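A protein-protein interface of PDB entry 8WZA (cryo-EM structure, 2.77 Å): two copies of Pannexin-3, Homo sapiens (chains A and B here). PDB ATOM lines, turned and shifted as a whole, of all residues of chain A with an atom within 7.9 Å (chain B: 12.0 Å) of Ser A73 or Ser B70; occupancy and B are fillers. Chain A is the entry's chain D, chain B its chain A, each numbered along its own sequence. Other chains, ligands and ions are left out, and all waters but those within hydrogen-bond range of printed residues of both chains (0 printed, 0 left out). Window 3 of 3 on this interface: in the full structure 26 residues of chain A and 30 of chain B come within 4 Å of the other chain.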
ATOM      1  N   SER A  68      19.489  10.772 -35.035  1.00  0.00           N
ATOM      2  CA  SER A  68      19.611  10.381 -33.643  1.00  0.00           C
ATOM      3  C   SER A  68      18.755   9.152 -33.358  1.00  0.00           C
ATOM      4  O   SER A  68      17.798   8.868 -34.085  1.00  0.00           O
ATOM      5  CB  SER A  68      19.200  11.537 -32.735  1.00  0.00           C
ATOM      6  OG  SER A  68      19.640  12.778 -33.258  1.00  0.00           O
ATOM      7  N   PRO A  69      19.086   8.392 -32.313  1.00  0.00           N
ATOM      8  CA  PRO A  69      18.257   7.233 -31.959  1.00  0.00           C
ATOM      9  C   PRO A  69      16.848   7.654 -31.568  1.00  0.00           C
ATOM     10  O   PRO A  69      16.619   8.753 -31.058  1.00  0.00           O
ATOM     11  CB  PRO A  69      19.002   6.605 -30.773  1.00  0.00           C
ATOM     12  CG  PRO A  69      19.980   7.637 -30.315  1.00  0.00           C
ATOM     13  CD  PRO A  69      20.317   8.459 -31.510  1.00  0.00           C
ATOM     14  N   SER A  70      15.893   6.755 -31.823  1.00  0.00           N
ATOM     15  CA  SER A  70      14.494   7.030 -31.514  1.00  0.00           C
ATOM     16  C   SER A  70      14.239   7.144 -30.016  1.00  0.00           C
ATOM     17  O   SER A  70      13.207   7.694 -29.618  1.00  0.00           O
ATOM     18  CB  SER A  70      13.602   5.942 -32.112  1.00  0.00           C
ATOM     19  OG  SER A  70      14.303   4.717 -32.231  1.00  0.00           O
ATOM     20  N   ASN A  71      15.147   6.631 -29.182  1.00  0.00           N
ATOM     21  CA  ASN A  71      15.002   6.786 -27.738  1.00  0.00           C
ATOM     22  C   ASN A  71      15.136   8.243 -27.314  1.00  0.00           C
ATOM     23  O   ASN A  71      14.598   8.636 -26.272  1.00  0.00           O
ATOM     24  CB  ASN A  71      16.040   5.929 -27.013  1.00  0.00           C
ATOM     25  CG  ASN A  71      15.422   4.752 -26.287  1.00  0.00           C
ATOM     26  OD1 ASN A  71      14.212   4.539 -26.341  1.00  0.00           O
ATOM     27  ND2 ASN A  71      16.256   3.977 -25.604  1.00  0.00           N
ATOM     28  N   PHE A  72      15.845   9.049 -28.098  1.00  0.00           N
ATOM     29  CA  PHE A  72      16.098  10.436 -27.739  1.00  0.00           C
ATOM     30  C   PHE A  72      14.811  11.252 -27.747  1.00  0.00           C
ATOM     31  O   PHE A  72      13.873  10.974 -28.499  1.00  0.00           O
ATOM     32  CB  PHE A  72      17.109  11.060 -28.703  1.00  0.00           C
ATOM     33  CG  PHE A  72      18.541  10.823 -28.320  1.00  0.00           C
ATOM     34  CD1 PHE A  72      18.904   9.705 -27.589  1.00  0.00           C
ATOM     35  CD2 PHE A  72      19.526  11.721 -28.694  1.00  0.00           C
ATOM     36  CE1 PHE A  72      20.221   9.488 -27.237  1.00  0.00           C
ATOM     37  CE2 PHE A  72      20.845  11.508 -28.346  1.00  0.00           C
ATOM     38  CZ  PHE A  72      21.192  10.391 -27.617  1.00  0.00           C
ATOM     39  N   SER A  73      14.775  12.268 -26.891  1.00  0.00           N
ATOM     40  CA  SER A  73      13.663  13.202 -26.859  1.00  0.00           C
ATOM     41  C   SER A  73      13.829  14.245 -27.962  1.00  0.00           C
ATOM     42  O   SER A  73      14.767  14.203 -28.762  1.00  0.00           O
ATOM     43  CB  SER A  73      13.565  13.862 -25.486  1.00  0.00           C
ATOM     44  OG  SER A  73      13.815  12.928 -24.452  1.00  0.00           O
ATOM     45  N   ILE A  74      12.894  15.193 -28.013  1.00  0.00           N
ATOM     46  CA  ILE A  74      13.000  16.280 -28.981  1.00  0.00           C
ATOM     47  C   ILE A  74      14.143  17.215 -28.608  1.00  0.00           C
ATOM     48  O   ILE A  74      14.930  17.635 -29.467  1.00  0.00           O
ATOM     49  CB  ILE A  74      11.658  17.029 -29.087  1.00  0.00           C
ATOM     50  CG1 ILE A  74      10.551  16.078 -29.548  1.00  0.00           C
ATOM     51  CG2 ILE A  74      11.776  18.207 -30.042  1.00  0.00           C
ATOM     52  CD1 ILE A  74       9.646  15.597 -28.431  1.00  0.00           C
ATOM     53  N   ARG A  75      14.263  17.543 -27.318  1.00  0.00           N
ATOM     54  CA  ARG A  75      15.314  18.454 -26.880  1.00  0.00           C
ATOM     55  C   ARG A  75      16.690  17.811 -26.990  1.00  0.00           C
ATOM     56  O   ARG A  75      17.670  18.486 -27.318  1.00  0.00           O
ATOM     57  CB  ARG A  75      15.044  18.912 -25.447  1.00  0.00           C
ATOM     58  CG  ARG A  75      13.723  19.641 -25.277  1.00  0.00           C
ATOM     59  CD  ARG A  75      13.921  21.144 -25.163  1.00  0.00           C
ATOM     60  NE  ARG A  75      14.744  21.678 -26.242  1.00  0.00           N
ATOM     61  CZ  ARG A  75      14.309  21.914 -27.473  1.00  0.00           C
ATOM     62  NH1 ARG A  75      13.060  21.662 -27.826  1.00  0.00           N
ATOM     63  NH2 ARG A  75      15.151  22.416 -28.372  1.00  0.00           N
ATOM     64  N   GLN A  76      16.787  16.507 -26.721  1.00  0.00           N
ATOM     65  CA  GLN A  76      18.066  15.821 -26.872  1.00  0.00           C
ATOM     66  C   GLN A  76      18.492  15.763 -28.336  1.00  0.00           C
ATOM     67  O   GLN A  76      19.676  15.934 -28.653  1.00  0.00           O
ATOM     68  CB  GLN A  76      17.979  14.422 -26.264  1.00  0.00           C
ATOM     69  CG  GLN A  76      17.904  14.431 -24.743  1.00  0.00           C
ATOM     70  CD  GLN A  76      17.882  13.040 -24.138  1.00  0.00           C
ATOM     71  OE1 GLN A  76      17.572  12.061 -24.815  1.00  0.00           O
ATOM     72  NE2 GLN A  76      18.209  12.949 -22.855  1.00  0.00           N
ATOM     73  N   ALA A  77      17.540  15.537 -29.244  1.00  0.00           N
ATOM     74  CA  ALA A  77      17.853  15.572 -30.669  1.00  0.00           C
ATOM     75  C   ALA A  77      18.280  16.969 -31.106  1.00  0.00           C
ATOM     76  O   ALA A  77      19.204  17.122 -31.916  1.00  0.00           O
ATOM     77  CB  ALA A  77      16.650  15.099 -31.483  1.00  0.00           C
ATOM     78  N   ALA A  78      17.613  18.002 -30.584  1.00  0.00           N
ATOM     79  CA  ALA A  78      18.018  19.372 -30.889  1.00  0.00           C
ATOM     80  C   ALA A  78      19.422  19.657 -30.371  1.00  0.00           C
ATOM     81  O   ALA A  78      20.212  20.335 -31.037  1.00  0.00           O
ATOM     82  CB  ALA A  78      17.015  20.361 -30.299  1.00  0.00           C
ATOM     83  N   TYR A  79      19.747  19.149 -29.179  1.00  0.00           N
ATOM     84  CA  TYR A  79      21.099  19.280 -28.648  1.00  0.00           C
ATOM     85  C   TYR A  79      22.112  18.599 -29.555  1.00  0.00           C
ATOM     86  O   TYR A  79      23.189  19.147 -29.821  1.00  0.00           O
ATOM     87  CB  TYR A  79      21.158  18.691 -27.235  1.00  0.00           C
ATOM     88  CG  TYR A  79      22.532  18.684 -26.592  1.00  0.00           C
ATOM     89  CD1 TYR A  79      23.431  17.648 -26.828  1.00  0.00           C
ATOM     90  CD2 TYR A  79      22.922  19.703 -25.733  1.00  0.00           C
ATOM     91  CE1 TYR A  79      24.681  17.637 -26.239  1.00  0.00           C
ATOM     92  CE2 TYR A  79      24.171  19.698 -25.139  1.00  0.00           C
ATOM     93  CZ  TYR A  79      25.045  18.663 -25.395  1.00  0.00           C
ATOM     94  OH  TYR A  79      26.288  18.656 -24.805  1.00  0.00           O
ATOM     95  N   VAL A  80      21.788  17.397 -30.035  1.00  0.00           N
ATOM     96  CA  VAL A  80      22.710  16.664 -30.898  1.00  0.00           C
ATOM     97  C   VAL A  80      22.950  17.431 -32.192  1.00  0.00           C
ATOM     98  O   VAL A  80      24.092  17.584 -32.642  1.00  0.00           O
ATOM     99  CB  VAL A  80      22.181  15.245 -31.170  1.00  0.00           C
ATOM    100  CG1 VAL A  80      22.913  14.620 -32.347  1.00  0.00           C
ATOM    101  CG2 VAL A  80      22.333  14.380 -29.933  1.00  0.00           C
ATOM    102  N   SER B  65      22.457  25.098 -25.225  1.00  0.00           N
ATOM    103  CA  SER B  65      21.754  23.828 -25.348  1.00  0.00           C
ATOM    104  C   SER B  65      22.034  22.980 -24.116  1.00  0.00           C
ATOM    105  O   SER B  65      23.133  23.025 -23.560  1.00  0.00           O
ATOM    106  CB  SER B  65      22.171  23.077 -26.616  1.00  0.00           C
ATOM    107  OG  SER B  65      21.201  23.230 -27.637  1.00  0.00           O
ATOM    108  N   CYS B  66      21.037  22.211 -23.686  1.00  0.00           N
ATOM    109  CA  CYS B  66      21.141  21.422 -22.468  1.00  0.00           C
ATOM    110  C   CYS B  66      20.782  19.971 -22.750  1.00  0.00           C
ATOM    111  O   CYS B  66      19.875  19.690 -23.538  1.00  0.00           O
ATOM    112  CB  CYS B  66      20.224  21.975 -21.372  1.00  0.00           C
ATOM    113  SG  CYS B  66      20.649  23.638 -20.824  1.00  0.00           S
ATOM    114  N   PHE B  67      21.501  19.054 -22.103  1.00  0.00           N
ATOM    115  CA  PHE B  67      21.196  17.627 -22.184  1.00  0.00           C
ATOM    116  C   PHE B  67      20.495  17.220 -20.891  1.00  0.00           C
ATOM    117  O   PHE B  67      21.095  16.684 -19.959  1.00  0.00           O
ATOM    118  CB  PHE B  67      22.464  16.815 -22.428  1.00  0.00           C
ATOM    119  CG  PHE B  67      22.224  15.525 -23.161  1.00  0.00           C
ATOM    120  CD1 PHE B  67      22.000  15.521 -24.527  1.00  0.00           C
ATOM    121  CD2 PHE B  67      22.223  14.316 -22.485  1.00  0.00           C
ATOM    122  CE1 PHE B  67      21.780  14.338 -25.205  1.00  0.00           C
ATOM    123  CE2 PHE B  67      22.003  13.130 -23.158  1.00  0.00           C
ATOM    124  CZ  PHE B  67      21.782  13.141 -24.520  1.00  0.00           C
ATOM    125  N   SER B  68      19.194  17.486 -20.845  1.00  0.00           N
ATOM    126  CA  SER B  68      18.377  17.122 -19.702  1.00  0.00           C
ATOM    127  C   SER B  68      17.973  15.654 -19.785  1.00  0.00           C
ATOM    128  O   SER B  68      17.962  15.062 -20.867  1.00  0.00           O
ATOM    129  CB  SER B  68      17.138  18.011 -19.641  1.00  0.00           C
ATOM    130  OG  SER B  68      17.447  19.344 -20.004  1.00  0.00           O
ATOM    131  N   PRO B  69      17.649  15.034 -18.649  1.00  0.00           N
ATOM    132  CA  PRO B  69      17.200  13.638 -18.678  1.00  0.00           C
ATOM    133  C   PRO B  69      15.905  13.483 -19.461  1.00  0.00           C
ATOM    134  O   PRO B  69      15.078  14.395 -19.529  1.00  0.00           O
ATOM    135  CB  PRO B  69      17.003  13.289 -17.197  1.00  0.00           C
ATOM    136  CG  PRO B  69      17.000  14.594 -16.470  1.00  0.00           C
ATOM    137  CD  PRO B  69      17.838  15.527 -17.274  1.00  0.00           C
ATOM    138  N   SER B  70      15.740  12.302 -20.063  1.00  0.00           N
ATOM    139  CA  SER B  70      14.557  12.022 -20.869  1.00  0.00           C
ATOM    140  C   SER B  70      13.279  11.981 -20.041  1.00  0.00           C
ATOM    141  O   SER B  70      12.186  12.094 -20.607  1.00  0.00           O
ATOM    142  CB  SER B  70      14.734  10.700 -21.617  1.00  0.00           C
ATOM    143  OG  SER B  70      15.614   9.836 -20.920  1.00  0.00           O
ATOM    144  N   ASN B  71      13.389  11.815 -18.721  1.00  0.00           N
ATOM    145  CA  ASN B  71      12.206  11.846 -17.868  1.00  0.00           C
ATOM    146  C   ASN B  71      11.577  13.234 -17.829  1.00  0.00           C
ATOM    147  O   ASN B  71      10.369  13.359 -17.593  1.00  0.00           O
ATOM    148  CB  ASN B  71      12.566  11.395 -16.452  1.00  0.00           C
ATOM    149  CG  ASN B  71      12.142   9.970 -16.168  1.00  0.00           C
ATOM    150  OD1 ASN B  71      11.666   9.262 -17.056  1.00  0.00           O
ATOM    151  ND2 ASN B  71      12.314   9.538 -14.925  1.00  0.00           N
ATOM    152  N   PHE B  72      12.372  14.276 -18.054  1.00  0.00           N
ATOM    153  CA  PHE B  72      11.877  15.643 -17.974  1.00  0.00           C
ATOM    154  C   PHE B  72      10.848  15.920 -19.062  1.00  0.00           C
ATOM    155  O   PHE B  72      10.891  15.349 -20.155  1.00  0.00           O
ATOM    156  CB  PHE B  72      13.034  16.636 -18.094  1.00  0.00           C
ATOM    157  CG  PHE B  72      13.730  16.924 -16.793  1.00  0.00           C
ATOM    158  CD1 PHE B  72      13.772  15.974 -15.786  1.00  0.00           C
ATOM    159  CD2 PHE B  72      14.345  18.146 -16.580  1.00  0.00           C
ATOM    160  CE1 PHE B  72      14.412  16.240 -14.591  1.00  0.00           C
ATOM    161  CE2 PHE B  72      14.988  18.416 -15.389  1.00  0.00           C
ATOM    162  CZ  PHE B  72      15.021  17.462 -14.393  1.00  0.00           C
ATOM    163  N   SER B  73       9.908  16.806 -18.747  1.00  0.00           N
ATOM    164  CA  SER B  73       8.918  17.246 -19.714  1.00  0.00           C
ATOM    165  C   SER B  73       9.516  18.320 -20.619  1.00  0.00           C
ATOM    166  O   SER B  73      10.688  18.689 -20.503  1.00  0.00           O
ATOM    167  CB  SER B  73       7.670  17.758 -19.000  1.00  0.00           C
ATOM    168  OG  SER B  73       7.354  16.947 -17.881  1.00  0.00           O
ATOM    169  N   ILE B  74       8.699  18.824 -21.544  1.00  0.00           N
ATOM    170  CA  ILE B  74       9.148  19.910 -22.409  1.00  0.00           C
ATOM    171  C   ILE B  74       9.323  21.192 -21.604  1.00  0.00           C
ATOM    172  O   ILE B  74      10.321  21.909 -21.755  1.00  0.00           O
ATOM    173  CB  ILE B  74       8.162  20.098 -23.577  1.00  0.00           C
ATOM    174  CG1 ILE B  74       8.096  18.827 -24.429  1.00  0.00           C
ATOM    175  CG2 ILE B  74       8.562  21.289 -24.432  1.00  0.00           C
ATOM    176  CD1 ILE B  74       6.873  17.971 -24.166  1.00  0.00           C
ATOM    177  N   ARG B  75       8.363  21.493 -20.725  1.00  0.00           N
ATOM    178  CA  ARG B  75       8.447  22.706 -19.921  1.00  0.00           C
ATOM    179  C   ARG B  75       9.578  22.623 -18.905  1.00  0.00           C
ATOM    180  O   ARG B  75      10.231  23.630 -18.615  1.00  0.00           O
ATOM    181  CB  ARG B  75       7.112  22.965 -19.224  1.00  0.00           C
ATOM    182  CG  ARG B  75       5.947  23.144 -20.183  1.00  0.00           C
ATOM    183  CD  ARG B  75       5.561  24.608 -20.330  1.00  0.00           C
ATOM    184  NE  ARG B  75       6.706  25.455 -20.640  1.00  0.00           N
ATOM    185  CZ  ARG B  75       7.262  25.561 -21.840  1.00  0.00           C
ATOM    186  NH1 ARG B  75       6.813  24.870 -22.873  1.00  0.00           N
ATOM    187  NH2 ARG B  75       8.296  26.381 -22.005  1.00  0.00           N
ATOM    188  N   GLN B  76       9.827  21.435 -18.353  1.00  0.00           N
ATOM    189  CA  GLN B  76      10.936  21.280 -17.416  1.00  0.00           C
ATOM    190  C   GLN B  76      12.280  21.461 -18.116  1.00  0.00           C
ATOM    191  O   GLN B  76      13.198  22.077 -17.562  1.00  0.00           O
ATOM    192  CB  GLN B  76      10.847  19.916 -16.730  1.00  0.00           C
ATOM    193  CG  GLN B  76       9.705  19.825 -15.726  1.00  0.00           C
ATOM    194  CD  GLN B  76       9.662  18.499 -14.993  1.00  0.00           C
ATOM    195  OE1 GLN B  76      10.222  17.504 -15.450  1.00  0.00           O
ATOM    196  NE2 GLN B  76       8.987  18.479 -13.849  1.00  0.00           N
ATOM    197  N   ALA B  77      12.411  20.944 -19.340  1.00  0.00           N
ATOM    198  CA  ALA B  77      13.629  21.171 -20.112  1.00  0.00           C
ATOM    199  C   ALA B  77      13.801  22.647 -20.449  1.00  0.00           C
ATOM    200  O   ALA B  77      14.920  23.178 -20.413  1.00  0.00           O
ATOM    201  CB  ALA B  77      13.609  20.326 -21.385  1.00  0.00           C
ATOM    202  N   ALA B  78      12.701  23.327 -20.787  1.00  0.00           N
ATOM    203  CA  ALA B  78      12.774  24.762 -21.046  1.00  0.00           C
ATOM    204  C   ALA B  78      13.193  25.525 -19.795  1.00  0.00           C
ATOM    205  O   ALA B  78      13.972  26.481 -19.874  1.00  0.00           O
ATOM    206  CB  ALA B  78      11.429  25.271 -21.564  1.00  0.00           C
ATOM    207  N   VAL B  80      15.084  24.296 -17.411  1.00  0.00           N
ATOM    208  CA  VAL B  80      16.498  23.999 -17.192  1.00  0.00           C
ATOM    209  C   VAL B  80      17.370  24.866 -18.093  1.00  0.00           C
ATOM    210  O   VAL B  80      18.361  25.454 -17.645  1.00  0.00           O
ATOM    211  CB  VAL B  80      16.773  22.500 -17.408  1.00  0.00           C
ATOM    212  CG1 VAL B  80      18.258  22.255 -17.600  1.00  0.00           C
ATOM    213  CG2 VAL B  80      16.251  21.693 -16.233  1.00  0.00           C
ATOM    214  N   THR B 253      14.102  15.356  -6.168  1.00  0.00           N
ATOM    215  CA  THR B 253      14.754  14.134  -6.631  1.00  0.00           C
ATOM    216  C   THR B 253      15.020  14.328  -8.121  1.00  0.00           C
ATOM    217  O   THR B 253      14.180  14.035  -8.976  1.00  0.00           O
ATOM    218  CB  THR B 253      13.915  12.885  -6.324  1.00  0.00           C
ATOM    219  OG1 THR B 253      14.133  12.518  -4.958  1.00  0.00           O
ATOM    220  CG2 THR B 253      14.350  11.704  -7.187  1.00  0.00           C
ATOM    221  N   HIS B 254      16.179  14.903  -8.413  1.00  0.00           N
ATOM    222  CA  HIS B 254      16.719  14.969  -9.760  1.00  0.00           C
ATOM    223  C   HIS B 254      18.198  15.294  -9.650  1.00  0.00           C
ATOM    224  O   HIS B 254      18.742  15.464  -8.553  1.00  0.00           O
ATOM    225  CB  HIS B 254      15.950  15.963 -10.641  1.00  0.00           C
ATOM    226  CG  HIS B 254      16.167  17.403 -10.296  1.00  0.00           C
ATOM    227  ND1 HIS B 254      15.238  18.129  -9.583  1.00  0.00           N
ATOM    228  CD2 HIS B 254      17.165  18.267 -10.602  1.00  0.00           C
ATOM    229  CE1 HIS B 254      15.661  19.372  -9.447  1.00  0.00           C
ATOM    230  NE2 HIS B 254      16.828  19.484 -10.055  1.00  0.00           N
ATOM    231  N   VAL B 255      18.844  15.389 -10.806  1.00  0.00           N
ATOM    232  CA  VAL B 255      20.297  15.436 -10.899  1.00  0.00           C
ATOM    233  C   VAL B 255      20.819  16.694 -10.212  1.00  0.00           C
ATOM    234  O   VAL B 255      20.427  17.823 -10.548  1.00  0.00           O
ATOM    235  CB  VAL B 255      20.744  15.421 -12.364  1.00  0.00           C
ATOM    236  CG1 VAL B 255      20.785  14.013 -12.916  1.00  0.00           C
ATOM    237  CG2 VAL B 255      19.839  16.335 -13.178  1.00  0.00           C
ATOM    238  N   ASN B 257      23.878  17.950 -10.736  1.00  0.00           N
ATOM    239  CA  ASN B 257      24.775  18.629 -11.659  1.00  0.00           C
ATOM    240  C   ASN B 257      24.265  18.375 -13.069  1.00  0.00           C
ATOM    241  O   ASN B 257      24.476  17.289 -13.616  1.00  0.00           O
ATOM    242  CB  ASN B 257      26.218  18.133 -11.502  1.00  0.00           C
ATOM    243  CG  ASN B 257      27.214  19.264 -11.287  1.00  0.00           C
ATOM    244  OD1 ASN B 257      26.830  20.429 -11.208  1.00  0.00           O
ATOM    245  ND2 ASN B 257      28.499  18.924 -11.195  1.00  0.00           N
ATOM    246  N   LEU B 258      23.586  19.361 -13.655  1.00  0.00           N
ATOM    247  CA  LEU B 258      23.084  19.207 -15.018  1.00  0.00           C
ATOM    248  C   LEU B 258      24.289  19.444 -15.920  1.00  0.00           C
ATOM    249  O   LEU B 258      24.539  20.542 -16.423  1.00  0.00           O
ATOM    250  CB  LEU B 258      21.924  20.162 -15.292  1.00  0.00           C
ATOM    251  CG  LEU B 258      21.098  20.158 -16.597  1.00  0.00           C
ATOM    252  CD1 LEU B 258      21.820  20.435 -17.923  1.00  0.00           C
ATOM    253  CD2 LEU B 258      20.362  18.827 -16.669  1.00  0.00           C
ATOM    254  N   ILE B 259      25.083  18.389 -16.073  1.00  0.00           N
ATOM    255  CA  ILE B 259      26.332  18.458 -16.817  1.00  0.00           C
ATOM    256  C   ILE B 259      26.029  18.731 -18.281  1.00  0.00           C
ATOM    257  O   ILE B 259      24.897  18.541 -18.741  1.00  0.00           O
ATOM    258  CB  ILE B 259      27.152  17.165 -16.654  1.00  0.00           C
ATOM    259  CG1 ILE B 259      26.450  16.001 -17.356  1.00  0.00           C
ATOM    260  CG2 ILE B 259      27.371  16.851 -15.180  1.00  0.00           C
ATOM    261  CD1 ILE B 259      27.196  14.691 -17.268  1.00  0.00           C
ATOM    262  N   THR B 260      27.045  19.170 -19.018  1.00  0.00           N
ATOM    263  CA  THR B 260      26.986  19.385 -20.465  1.00  0.00           C
ATOM    264  C   THR B 260      25.830  20.306 -20.863  1.00  0.00           C
ATOM    265  O   THR B 260      24.848  19.906 -21.488  1.00  0.00           O
ATOM    266  CB  THR B 260      26.925  18.064 -21.238  1.00  0.00           C
ATOM    267  OG1 THR B 260      26.155  17.090 -20.525  1.00  0.00           O
ATOM    268  CG2 THR B 260      28.326  17.547 -21.459  1.00  0.00           C
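The backbone carbonyl oxygen of Ser B68 lies within hydrogen-bond range of the side-chain amide nitrogen of Gln A76 (2.9 Å).
N of Ser A73 is in hydrogen-bond range of OE1 of Gln A76, 3.5 Å away.
Among the printed residues, pairs that only touch across the chains: Tyr A79 with Phe B67 (3.4 Å), Tyr A79 with Ser B65 (3.6 Å), Tyr A79 with Thr B260 (3.7 Å), Tyr A79 with Cys B66 (3.7 Å), Ser A73 with Ser B70 (3.7 Å), Gln A76 with Ser B70 (3.8 Å), Gln A76 with Phe B67 (3.8 Å) and Arg A75 with Ala B77 (3.9 Å).
No residue of chain B comes within 4 Å of Phe A72.
Of chain B, only Ser B70 (3.7 Å) comes within 4 Å of Ser A73.
No residue of chain B comes within 4 Å of Ile A74.
Printed residues of chain B within 4 Å of Gln A76: Phe B67, Ser B68 and Ser B70.
Of the printed residues of chain B, Tyr A79 touches Ser B65 (3.6 Å), Cys B66 (3.7 Å), Phe B67 (3.4 Å) and Thr B260 (3.7 Å).
Of the printed residues of chain A, Ser B65 touches Tyr A79 (3.6 Å).
Of chain A, only Ser A73 and Gln A76 come within 4 Å of Ser B70.
Ser B73 touches none of the printed residues of chain A.
Ile B259 touches none of the printed residues of chain A.
The nearest residue of chain A that does not touch Ser B70 is Asn A71 (5.1 Å).
The nearest printed residue of chain A that does not touch Ser B68 is Ser A73 (5.9 Å).
Of the 22 printed residues of chain B, 7 touch a printed residue of chain A.
Of the 13 printed residues of chain A, 4 touch a printed residue of chain B.
Hydrophobic or aromatic side chains of chain A within 4 Å of the printed part of chain B: Tyr A79.
Among the printed residues, 9 pairs touch across the chains.
Among the printed residues, no Asp or Glu carboxylate lies within 4 Å of a Lys or Arg side-chain nitrogen of the other chain.
Ser A73 touches Ser B70, but with the chains exchanged Ser A70 does not touch Ser B73 (14.4 Å).
Arg A75 touches Ala B77, but with the chains exchanged Ala A77 does not touch Arg B75 (13.9 Å).
Gln A76 touches Ser B68, but with the chains exchanged Ser A68 does not touch Gln B76 (18.9 Å).
Gln A76 touches Ser B70, but with the chains exchanged Ser A70 does not touch Gln B76 (17.5 Å).
Positions printed for both chains: 68, 69, 70, 71, 72, 73, 74, 75, 76, 77, 78 and 80.
Of the 9 pairs that touch across the chains among the printed residues, none has its exchanged pair printed and touching as well.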
